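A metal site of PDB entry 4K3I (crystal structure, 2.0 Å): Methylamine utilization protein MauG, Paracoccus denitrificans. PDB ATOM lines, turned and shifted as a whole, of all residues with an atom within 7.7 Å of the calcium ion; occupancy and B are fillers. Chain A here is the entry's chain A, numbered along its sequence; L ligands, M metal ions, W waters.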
ATOM      1  N   ARG A  39      17.345  -9.945  35.572  1.00  0.00           N
ATOM      2  CA  ARG A  39      18.273 -10.241  34.507  1.00  0.00           C
ATOM      3  C   ARG A  39      18.743  -9.001  33.745  1.00  0.00           C
ATOM      4  O   ARG A  39      18.717  -8.966  32.531  1.00  0.00           O
ATOM      5  CB  ARG A  39      17.591 -11.239  33.565  1.00  0.00           C
ATOM      6  CG  ARG A  39      18.545 -11.855  32.585  1.00  0.00           C
ATOM      7  CD  ARG A  39      17.827 -12.790  31.612  1.00  0.00           C
ATOM      8  NE  ARG A  39      18.755 -13.767  30.985  1.00  0.00           N
ATOM      9  CZ  ARG A  39      19.390 -13.590  29.839  1.00  0.00           C
ATOM     10  NH1 ARG A  39      20.188 -14.542  29.370  1.00  0.00           N
ATOM     11  NH2 ARG A  39      19.282 -12.455  29.145  1.00  0.00           N
ATOM     12  N   THR A  42      16.232  -7.798  30.951  1.00  0.00           N
ATOM     13  CA  THR A  42      16.123  -8.556  29.727  1.00  0.00           C
ATOM     14  C   THR A  42      15.265  -9.794  30.000  1.00  0.00           C
ATOM     15  O   THR A  42      14.768  -9.940  31.107  1.00  0.00           O
ATOM     16  CB  THR A  42      17.505  -8.887  29.156  1.00  0.00           C
ATOM     17  OG1 THR A  42      18.175  -9.779  30.012  1.00  0.00           O
ATOM     18  CG2 THR A  42      18.311  -7.638  29.014  1.00  0.00           C
ATOM     19  N   ASP A  43      14.999 -10.593  28.983  1.00  0.00           N
ATOM     20  CA  ASP A  43      14.026 -11.667  29.043  1.00  0.00           C
ATOM     21  C   ASP A  43      14.637 -13.057  29.233  1.00  0.00           C
ATOM     22  O   ASP A  43      15.281 -13.588  28.340  1.00  0.00           O
ATOM     23  CB  ASP A  43      13.128 -11.595  27.816  1.00  0.00           C
ATOM     24  CG  ASP A  43      11.887 -12.522  27.888  1.00  0.00           C
ATOM     25  OD1 ASP A  43      11.721 -13.274  28.876  1.00  0.00           O
ATOM     26  OD2 ASP A  43      11.135 -12.535  26.861  1.00  0.00           O
ATOM     27  N   LEU A  51      16.438 -17.850  23.695  1.00  0.00           N
ATOM     28  CA  LEU A  51      16.294 -16.528  24.292  1.00  0.00           C
ATOM     29  C   LEU A  51      16.465 -15.402  23.251  1.00  0.00           C
ATOM     30  O   LEU A  51      16.517 -14.183  23.559  1.00  0.00           O
ATOM     31  CB  LEU A  51      17.236 -16.389  25.458  1.00  0.00           C
ATOM     32  CG  LEU A  51      16.757 -16.862  26.859  1.00  0.00           C
ATOM     33  CD1 LEU A  51      16.363 -18.280  26.884  1.00  0.00           C
ATOM     34  CD2 LEU A  51      17.877 -16.749  27.882  1.00  0.00           C
ATOM     35  N   ALA A  52      16.505 -15.778  21.993  1.00  0.00           N
ATOM     36  CA  ALA A  52      16.841 -14.757  20.987  1.00  0.00           C
ATOM     37  C   ALA A  52      15.751 -13.692  20.846  1.00  0.00           C
ATOM     38  O   ALA A  52      16.056 -12.542  20.619  1.00  0.00           O
ATOM     39  CB  ALA A  52      17.088 -15.423  19.638  1.00  0.00           C
ATOM     40  N   ASN A  66      15.873  -9.117  19.490  1.00  0.00           N
ATOM     41  CA  ASN A  66      16.186  -9.437  20.878  1.00  0.00           C
ATOM     42  C   ASN A  66      15.769  -8.300  21.789  1.00  0.00           C
ATOM     43  O   ASN A  66      16.012  -7.086  21.517  1.00  0.00           O
ATOM     44  CB  ASN A  66      17.686  -9.695  20.969  1.00  0.00           C
ATOM     45  CG  ASN A  66      18.188 -10.091  22.353  1.00  0.00           C
ATOM     46  OD1 ASN A  66      18.987  -9.387  22.929  1.00  0.00           O
ATOM     47  ND2 ASN A  66      17.783 -11.258  22.836  1.00  0.00           N
ATOM     48  N   THR A  67      15.173  -8.651  22.906  1.00  0.00           N
ATOM     49  CA  THR A  67      14.779  -7.650  23.929  1.00  0.00           C
ATOM     50  C   THR A  67      16.034  -7.075  24.586  1.00  0.00           C
ATOM     51  O   THR A  67      16.806  -7.831  25.252  1.00  0.00           O
ATOM     52  CB  THR A  67      13.881  -8.340  24.973  1.00  0.00           C
ATOM     53  OG1 THR A  67      12.686  -8.784  24.321  1.00  0.00           O
ATOM     54  CG2 THR A  67      13.557  -7.407  26.216  1.00  0.00           C
ATOM     55  N   PRO A  68      16.276  -5.761  24.404  1.00  0.00           N
ATOM     56  CA  PRO A  68      17.421  -5.122  24.999  1.00  0.00           C
ATOM     57  C   PRO A  68      17.188  -4.759  26.406  1.00  0.00           C
ATOM     58  O   PRO A  68      16.012  -4.601  26.850  1.00  0.00           O
ATOM     59  CB  PRO A  68      17.585  -3.837  24.193  1.00  0.00           C
ATOM     60  CG  PRO A  68      16.140  -3.443  23.895  1.00  0.00           C
ATOM     61  CD  PRO A  68      15.428  -4.767  23.686  1.00  0.00           C
ATOM     62  N   THR A  69      18.304  -4.629  27.114  1.00  0.00           N
ATOM     63  CA  THR A  69      18.287  -4.041  28.448  1.00  0.00           C
ATOM     64  C   THR A  69      17.735  -2.644  28.485  1.00  0.00           C
ATOM     65  O   THR A  69      17.938  -1.806  27.541  1.00  0.00           O
ATOM     66  CB  THR A  69      19.696  -4.059  29.107  1.00  0.00           C
ATOM     67  OG1 THR A  69      19.624  -3.684  30.462  1.00  0.00           O
ATOM     68  CG2 THR A  69      20.613  -3.044  28.427  1.00  0.00           C
ATOM     69  N   TRP A  93      16.282  -0.669  18.518  1.00  0.00           N
ATOM     70  CA  TRP A  93      17.513  -1.004  17.842  1.00  0.00           C
ATOM     71  C   TRP A  93      17.629  -0.221  16.507  1.00  0.00           C
ATOM     72  O   TRP A  93      18.737  -0.087  15.990  1.00  0.00           O
ATOM     73  CB  TRP A  93      17.541  -2.482  17.506  1.00  0.00           C
ATOM     74  CG  TRP A  93      17.768  -3.431  18.618  1.00  0.00           C
ATOM     75  CD1 TRP A  93      16.819  -4.192  19.262  1.00  0.00           C
ATOM     76  CD2 TRP A  93      19.013  -3.882  19.069  1.00  0.00           C
ATOM     77  NE1 TRP A  93      17.429  -5.044  20.167  1.00  0.00           N
ATOM     78  CE2 TRP A  93      18.782  -4.867  20.073  1.00  0.00           C
ATOM     79  CE3 TRP A  93      20.334  -3.564  18.725  1.00  0.00           C
ATOM     80  CZ2 TRP A  93      19.831  -5.533  20.745  1.00  0.00           C
ATOM     81  CZ3 TRP A  93      21.371  -4.203  19.391  1.00  0.00           C
ATOM     82  CH2 TRP A  93      21.104  -5.190  20.391  1.00  0.00           C
ATOM     83  N   VAL A 272      26.672  -6.386  29.575  1.00  0.00           N
ATOM     84  CA  VAL A 272      26.672  -7.238  28.415  1.00  0.00           C
ATOM     85  C   VAL A 272      26.927  -8.672  28.829  1.00  0.00           C
ATOM     86  O   VAL A 272      26.396  -9.612  28.261  1.00  0.00           O
ATOM     87  CB  VAL A 272      27.715  -6.787  27.390  1.00  0.00           C
ATOM     88  CG1 VAL A 272      29.154  -6.934  27.902  1.00  0.00           C
ATOM     89  CG2 VAL A 272      27.534  -7.550  26.106  1.00  0.00           C
ATOM     90  N   VAL A 274      25.726 -10.364  31.112  1.00  0.00           N
ATOM     91  CA  VAL A 274      24.608 -11.104  31.668  1.00  0.00           C
ATOM     92  C   VAL A 274      23.315 -10.942  30.814  1.00  0.00           C
ATOM     93  O   VAL A 274      22.248 -11.451  31.211  1.00  0.00           O
ATOM     94  CB  VAL A 274      24.300 -10.704  33.160  1.00  0.00           C
ATOM     95  CG1 VAL A 274      25.515 -10.960  34.047  1.00  0.00           C
ATOM     96  CG2 VAL A 274      23.907  -9.230  33.295  1.00  0.00           C
ATOM     97  N   THR A 275      23.431 -10.414  29.612  1.00  0.00           N
ATOM     98  CA  THR A 275      22.241 -10.111  28.788  1.00  0.00           C
ATOM     99  C   THR A 275      22.295 -10.809  27.436  1.00  0.00           C
ATOM    100  O   THR A 275      21.638 -10.387  26.473  1.00  0.00           O
ATOM    101  CB  THR A 275      22.063  -8.589  28.487  1.00  0.00           C
ATOM    102  OG1 THR A 275      23.247  -8.107  27.840  1.00  0.00           O
ATOM    103  CG2 THR A 275      21.843  -7.898  29.768  1.00  0.00           C
ATOM    104  N   GLY A 276      23.017 -11.938  27.381  1.00  0.00           N
ATOM    105  CA  GLY A 276      22.914 -12.807  26.199  1.00  0.00           C
ATOM    106  C   GLY A 276      21.496 -13.294  25.948  1.00  0.00           C
ATOM    107  O   GLY A 276      20.668 -13.265  26.855  1.00  0.00           O
ATOM    108  N   PRO A 277      21.216 -13.770  24.710  1.00  0.00           N
ATOM    109  CA  PRO A 277      22.093 -13.788  23.575  1.00  0.00           C
ATOM    110  C   PRO A 277      22.259 -12.362  22.929  1.00  0.00           C
ATOM    111  O   PRO A 277      21.709 -11.378  23.394  1.00  0.00           O
ATOM    112  CB  PRO A 277      21.418 -14.755  22.607  1.00  0.00           C
ATOM    113  CG  PRO A 277      19.971 -14.628  22.914  1.00  0.00           C
ATOM    114  CD  PRO A 277      19.901 -14.341  24.392  1.00  0.00           C
ATOM    115  N   TYR A 278      23.080 -12.286  21.899  1.00  0.00           N
ATOM    116  CA  TYR A 278      23.731 -10.970  21.553  1.00  0.00           C
ATOM    117  C   TYR A 278      23.290 -10.524  20.148  1.00  0.00           C
ATOM    118  O   TYR A 278      22.928 -11.362  19.359  1.00  0.00           O
ATOM    119  CB  TYR A 278      25.254 -11.092  21.636  1.00  0.00           C
ATOM    120  CG  TYR A 278      25.694 -11.325  23.065  1.00  0.00           C
ATOM    121  CD1 TYR A 278      25.532 -10.361  24.005  1.00  0.00           C
ATOM    122  CD2 TYR A 278      26.141 -12.562  23.496  1.00  0.00           C
ATOM    123  CE1 TYR A 278      25.809 -10.595  25.317  1.00  0.00           C
ATOM    124  CE2 TYR A 278      26.393 -12.814  24.830  1.00  0.00           C
ATOM    125  CZ  TYR A 278      26.252 -11.827  25.726  1.00  0.00           C
ATOM    126  OH  TYR A 278      26.513 -12.000  27.046  1.00  0.00           O
ATOM    127  N   MET A 279      23.510  -9.245  19.849  1.00  0.00           N
ATOM    128  CA  MET A 279      23.061  -8.594  18.639  1.00  0.00           C
ATOM    129  C   MET A 279      21.578  -8.398  18.541  1.00  0.00           C
ATOM    130  O   MET A 279      20.818  -8.886  19.373  1.00  0.00           O
ATOM    131  CB  MET A 279      23.641  -9.270  17.428  1.00  0.00           C
ATOM    132  CG  MET A 279      25.138  -9.492  17.583  1.00  0.00           C
ATOM    133  SD  MET A 279      26.091  -7.944  17.683  1.00  0.00           S
ATOM    134  CE  MET A 279      27.728  -8.656  17.918  1.00  0.00           C
ATOM    135  N   HIS A 280      21.171  -7.637  17.533  1.00  0.00           N
ATOM    136  CA  HIS A 280      19.794  -7.216  17.465  1.00  0.00           C
ATOM    137  C   HIS A 280      18.820  -8.320  17.300  1.00  0.00           C
ATOM    138  O   HIS A 280      17.630  -8.099  17.487  1.00  0.00           O
ATOM    139  CB  HIS A 280      19.612  -6.209  16.337  1.00  0.00           C
ATOM    140  CG  HIS A 280      19.838  -6.786  14.967  1.00  0.00           C
ATOM    141  ND1 HIS A 280      20.969  -6.523  14.223  1.00  0.00           N
ATOM    142  CD2 HIS A 280      19.055  -7.576  14.201  1.00  0.00           C
ATOM    143  CE1 HIS A 280      20.872  -7.137  13.061  1.00  0.00           C
ATOM    144  NE2 HIS A 280      19.722  -7.765  13.017  1.00  0.00           N
ATOM    145  N   ASN A 281      19.318  -9.451  16.843  1.00  0.00           N
ATOM    146  CA  ASN A 281      18.552 -10.651  16.649  1.00  0.00           C
ATOM    147  C   ASN A 281      18.887 -11.818  17.502  1.00  0.00           C
ATOM    148  O   ASN A 281      18.391 -12.928  17.287  1.00  0.00           O
ATOM    149  CB  ASN A 281      18.544 -11.067  15.178  1.00  0.00           C
ATOM    150  CG  ASN A 281      19.913 -11.312  14.672  1.00  0.00           C
ATOM    151  OD1 ASN A 281      20.852 -11.434  15.473  1.00  0.00           O
ATOM    152  ND2 ASN A 281      20.058 -11.416  13.354  1.00  0.00           N
ATOM    153  N   GLY A 282      19.693 -11.621  18.511  1.00  0.00           N
ATOM    154  CA  GLY A 282      19.958 -12.738  19.446  1.00  0.00           C
ATOM    155  C   GLY A 282      20.765 -13.866  18.869  1.00  0.00           C
ATOM    156  O   GLY A 282      20.710 -14.984  19.371  1.00  0.00           O
ATOM    157  N   PHE A 284      23.944 -14.779  18.496  1.00  0.00           N
ATOM    158  CA  PHE A 284      25.032 -15.413  19.222  1.00  0.00           C
ATOM    159  C   PHE A 284      24.699 -15.640  20.685  1.00  0.00           C
ATOM    160  O   PHE A 284      24.475 -14.749  21.412  1.00  0.00           O
ATOM    161  CB  PHE A 284      26.322 -14.581  19.156  1.00  0.00           C
ATOM    162  CG  PHE A 284      26.720 -14.197  17.768  1.00  0.00           C
ATOM    163  CD1 PHE A 284      26.665 -15.121  16.738  1.00  0.00           C
ATOM    164  CD2 PHE A 284      27.107 -12.899  17.473  1.00  0.00           C
ATOM    165  CE1 PHE A 284      26.989 -14.753  15.445  1.00  0.00           C
ATOM    166  CE2 PHE A 284      27.475 -12.539  16.190  1.00  0.00           C
ATOM    167  CZ  PHE A 284      27.383 -13.441  15.198  1.00  0.00           C
HETATM  168 FE1  LIG L   1      30.456  -3.932  18.735  1.00  0.00          FE
HETATM  169  C1  LIG L   1      27.357  -5.106  19.257  1.00  0.00           C
HETATM  170  C2  LIG L   1      31.651  -5.765  21.266  1.00  0.00           C
HETATM  171  C3  LIG L   1      33.629  -3.208  17.595  1.00  0.00           C
HETATM  172  C4  LIG L   1      29.233  -1.584  16.671  1.00  0.00           C
HETATM  173  N1  LIG L   1      29.618  -5.206  20.018  1.00  0.00           N
HETATM  174  C5  LIG L   1      28.356  -5.623  20.051  1.00  0.00           C
HETATM  175  C6  LIG L   1      28.100  -6.615  21.099  1.00  0.00           C
HETATM  176  C7  LIG L   1      29.322  -6.827  21.667  1.00  0.00           C
HETATM  177  C8  LIG L   1      30.208  -5.891  21.000  1.00  0.00           C
HETATM  178  C9  LIG L   1      29.712  -7.722  22.848  1.00  0.00           C
HETATM  179  C10 LIG L   1      26.770  -7.212  21.404  1.00  0.00           C
HETATM  180  C11 LIG L   1      26.069  -6.362  22.498  1.00  0.00           C
HETATM  181  C12 LIG L   1      24.588  -6.721  22.719  1.00  0.00           C
HETATM  182  O1  LIG L   1      23.997  -7.492  21.922  1.00  0.00           O
HETATM  183  O2  LIG L   1      23.993  -6.233  23.748  1.00  0.00           O
HETATM  184  N2  LIG L   1      32.328  -4.414  19.332  1.00  0.00           N
HETATM  185  C13 LIG L   1      32.607  -5.103  20.421  1.00  0.00           C
HETATM  186  C14 LIG L   1      34.036  -5.347  20.567  1.00  0.00           C
HETATM  187  C15 LIG L   1      34.638  -4.592  19.570  1.00  0.00           C
HETATM  188  C16 LIG L   1      33.500  -4.053  18.806  1.00  0.00           C
HETATM  189  C17 LIG L   1      34.649  -6.092  21.744  1.00  0.00           C
HETATM  190  C18 LIG L   1      36.117  -4.500  19.271  1.00  0.00           C
HETATM  191  C19 LIG L   1      36.619  -5.967  18.973  1.00  0.00           C
HETATM  192  N3  LIG L   1      31.287  -2.653  17.416  1.00  0.00           N
HETATM  193  C20 LIG L   1      32.539  -2.499  17.042  1.00  0.00           C
HETATM  194  C21 LIG L   1      32.781  -1.463  16.039  1.00  0.00           C
HETATM  195  C22 LIG L   1      31.524  -0.968  15.824  1.00  0.00           C
HETATM  196  C23 LIG L   1      30.637  -1.775  16.666  1.00  0.00           C
HETATM  197  C24 LIG L   1      34.134  -1.068  15.506  1.00  0.00           C
HETATM  198  C25 LIG L   1      31.235   0.121  14.889  1.00  0.00           C
HETATM  199  C26 LIG L   1      31.793  -0.134  13.518  1.00  0.00           C
HETATM  200  N4  LIG L   1      28.581  -3.397  18.127  1.00  0.00           N
HETATM  201  C27 LIG L   1      28.292  -2.480  17.225  1.00  0.00           C
HETATM  202  C28 LIG L   1      26.886  -2.449  16.829  1.00  0.00           C
HETATM  203  C29 LIG L   1      26.351  -3.503  17.539  1.00  0.00           C
HETATM  204  C30 LIG L   1      27.463  -4.012  18.324  1.00  0.00           C
HETATM  205  C31 LIG L   1      26.172  -1.568  15.810  1.00  0.00           C
HETATM  206  C32 LIG L   1      24.954  -3.980  17.399  1.00  0.00           C
HETATM  207  C33 LIG L   1      24.995  -4.793  16.109  1.00  0.00           C
HETATM  208  C34 LIG L   1      23.638  -5.337  15.757  1.00  0.00           C
HETATM  209  O3  LIG L   1      23.058  -6.016  16.661  1.00  0.00           O
HETATM  210  O4  LIG L   1      23.164  -5.124  14.588  1.00  0.00           O
HETATM  211 CA    CA M   1      20.772  -9.516  24.447  1.00  0.00          CA
HETATM  212  O   HOH W   1      19.145 -11.179  25.360  1.00  0.00           O
HETATM  213  O   HOH W   2      22.714  -8.167  25.104  1.00  0.00           O
HETATM  214  O   HOH W   3      19.524  -8.060  25.602  1.00  0.00           O
HETATM  215  O   HOH W   4      21.425  -8.271  22.466  1.00  0.00           O
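An oxygen (O3) of the ligand lies within hydrogen-bond range of the backbone NH of His 280, at 2.6 Å.
An oxygen (O1) of the ligand is in hydrogen-bond range of the backbone NH of Met 279.
ND1 of His 280 is in hydrogen-bond range of O4 of the ligand, 2.6 Å away.
O of Ala 52 is in hydrogen-bond range of ND2 of Asn 66 (3.1 Å).
O of Leu 51 lies within hydrogen-bond range of ND2 of Asn 66 (3.3 Å).
The backbone carbonyl oxygen of Asn 66 lies within hydrogen-bond range of the indole nitrogen of Trp 93.
The backbone NH (N) of Asn 66 sits at hydrogen-bond distance from the backbone carbonyl oxygen (O) of His 280 (2.9 Å).
Water W2 bridges O2 of the ligand (2.7 Å) and OG1 of Thr 275 (2.8 Å).
Water W4 lies within hydrogen-bond range of an oxygen (O1) of the ligand (2.7 Å) and the backbone carbonyl oxygen (O) of Met 279 (3.2 Å).
Water W1 lies within hydrogen-bond range of ND2 of Asn 66 (2.9 Å) and O of Gly 276 (3.0 Å).
The nearest printed residue that does not touch the calcium ion is Gly 276 (4.1 Å).
Water W3 binds the calcium ion (2.2 Å).
The calcium ion is bound by O of Pro 277, 2.3 Å away.
The calcium ion is bound by OD1 of Asn 66, 2.3 Å away.
O of Thr 275 is bound to the calcium ion (2.4 Å).
Water W4 is bound to the calcium ion, at 2.4 Å.
Water W2 binds the calcium ion (2.5 Å).
The calcium ion is bound by water W1 (2.5 Å).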
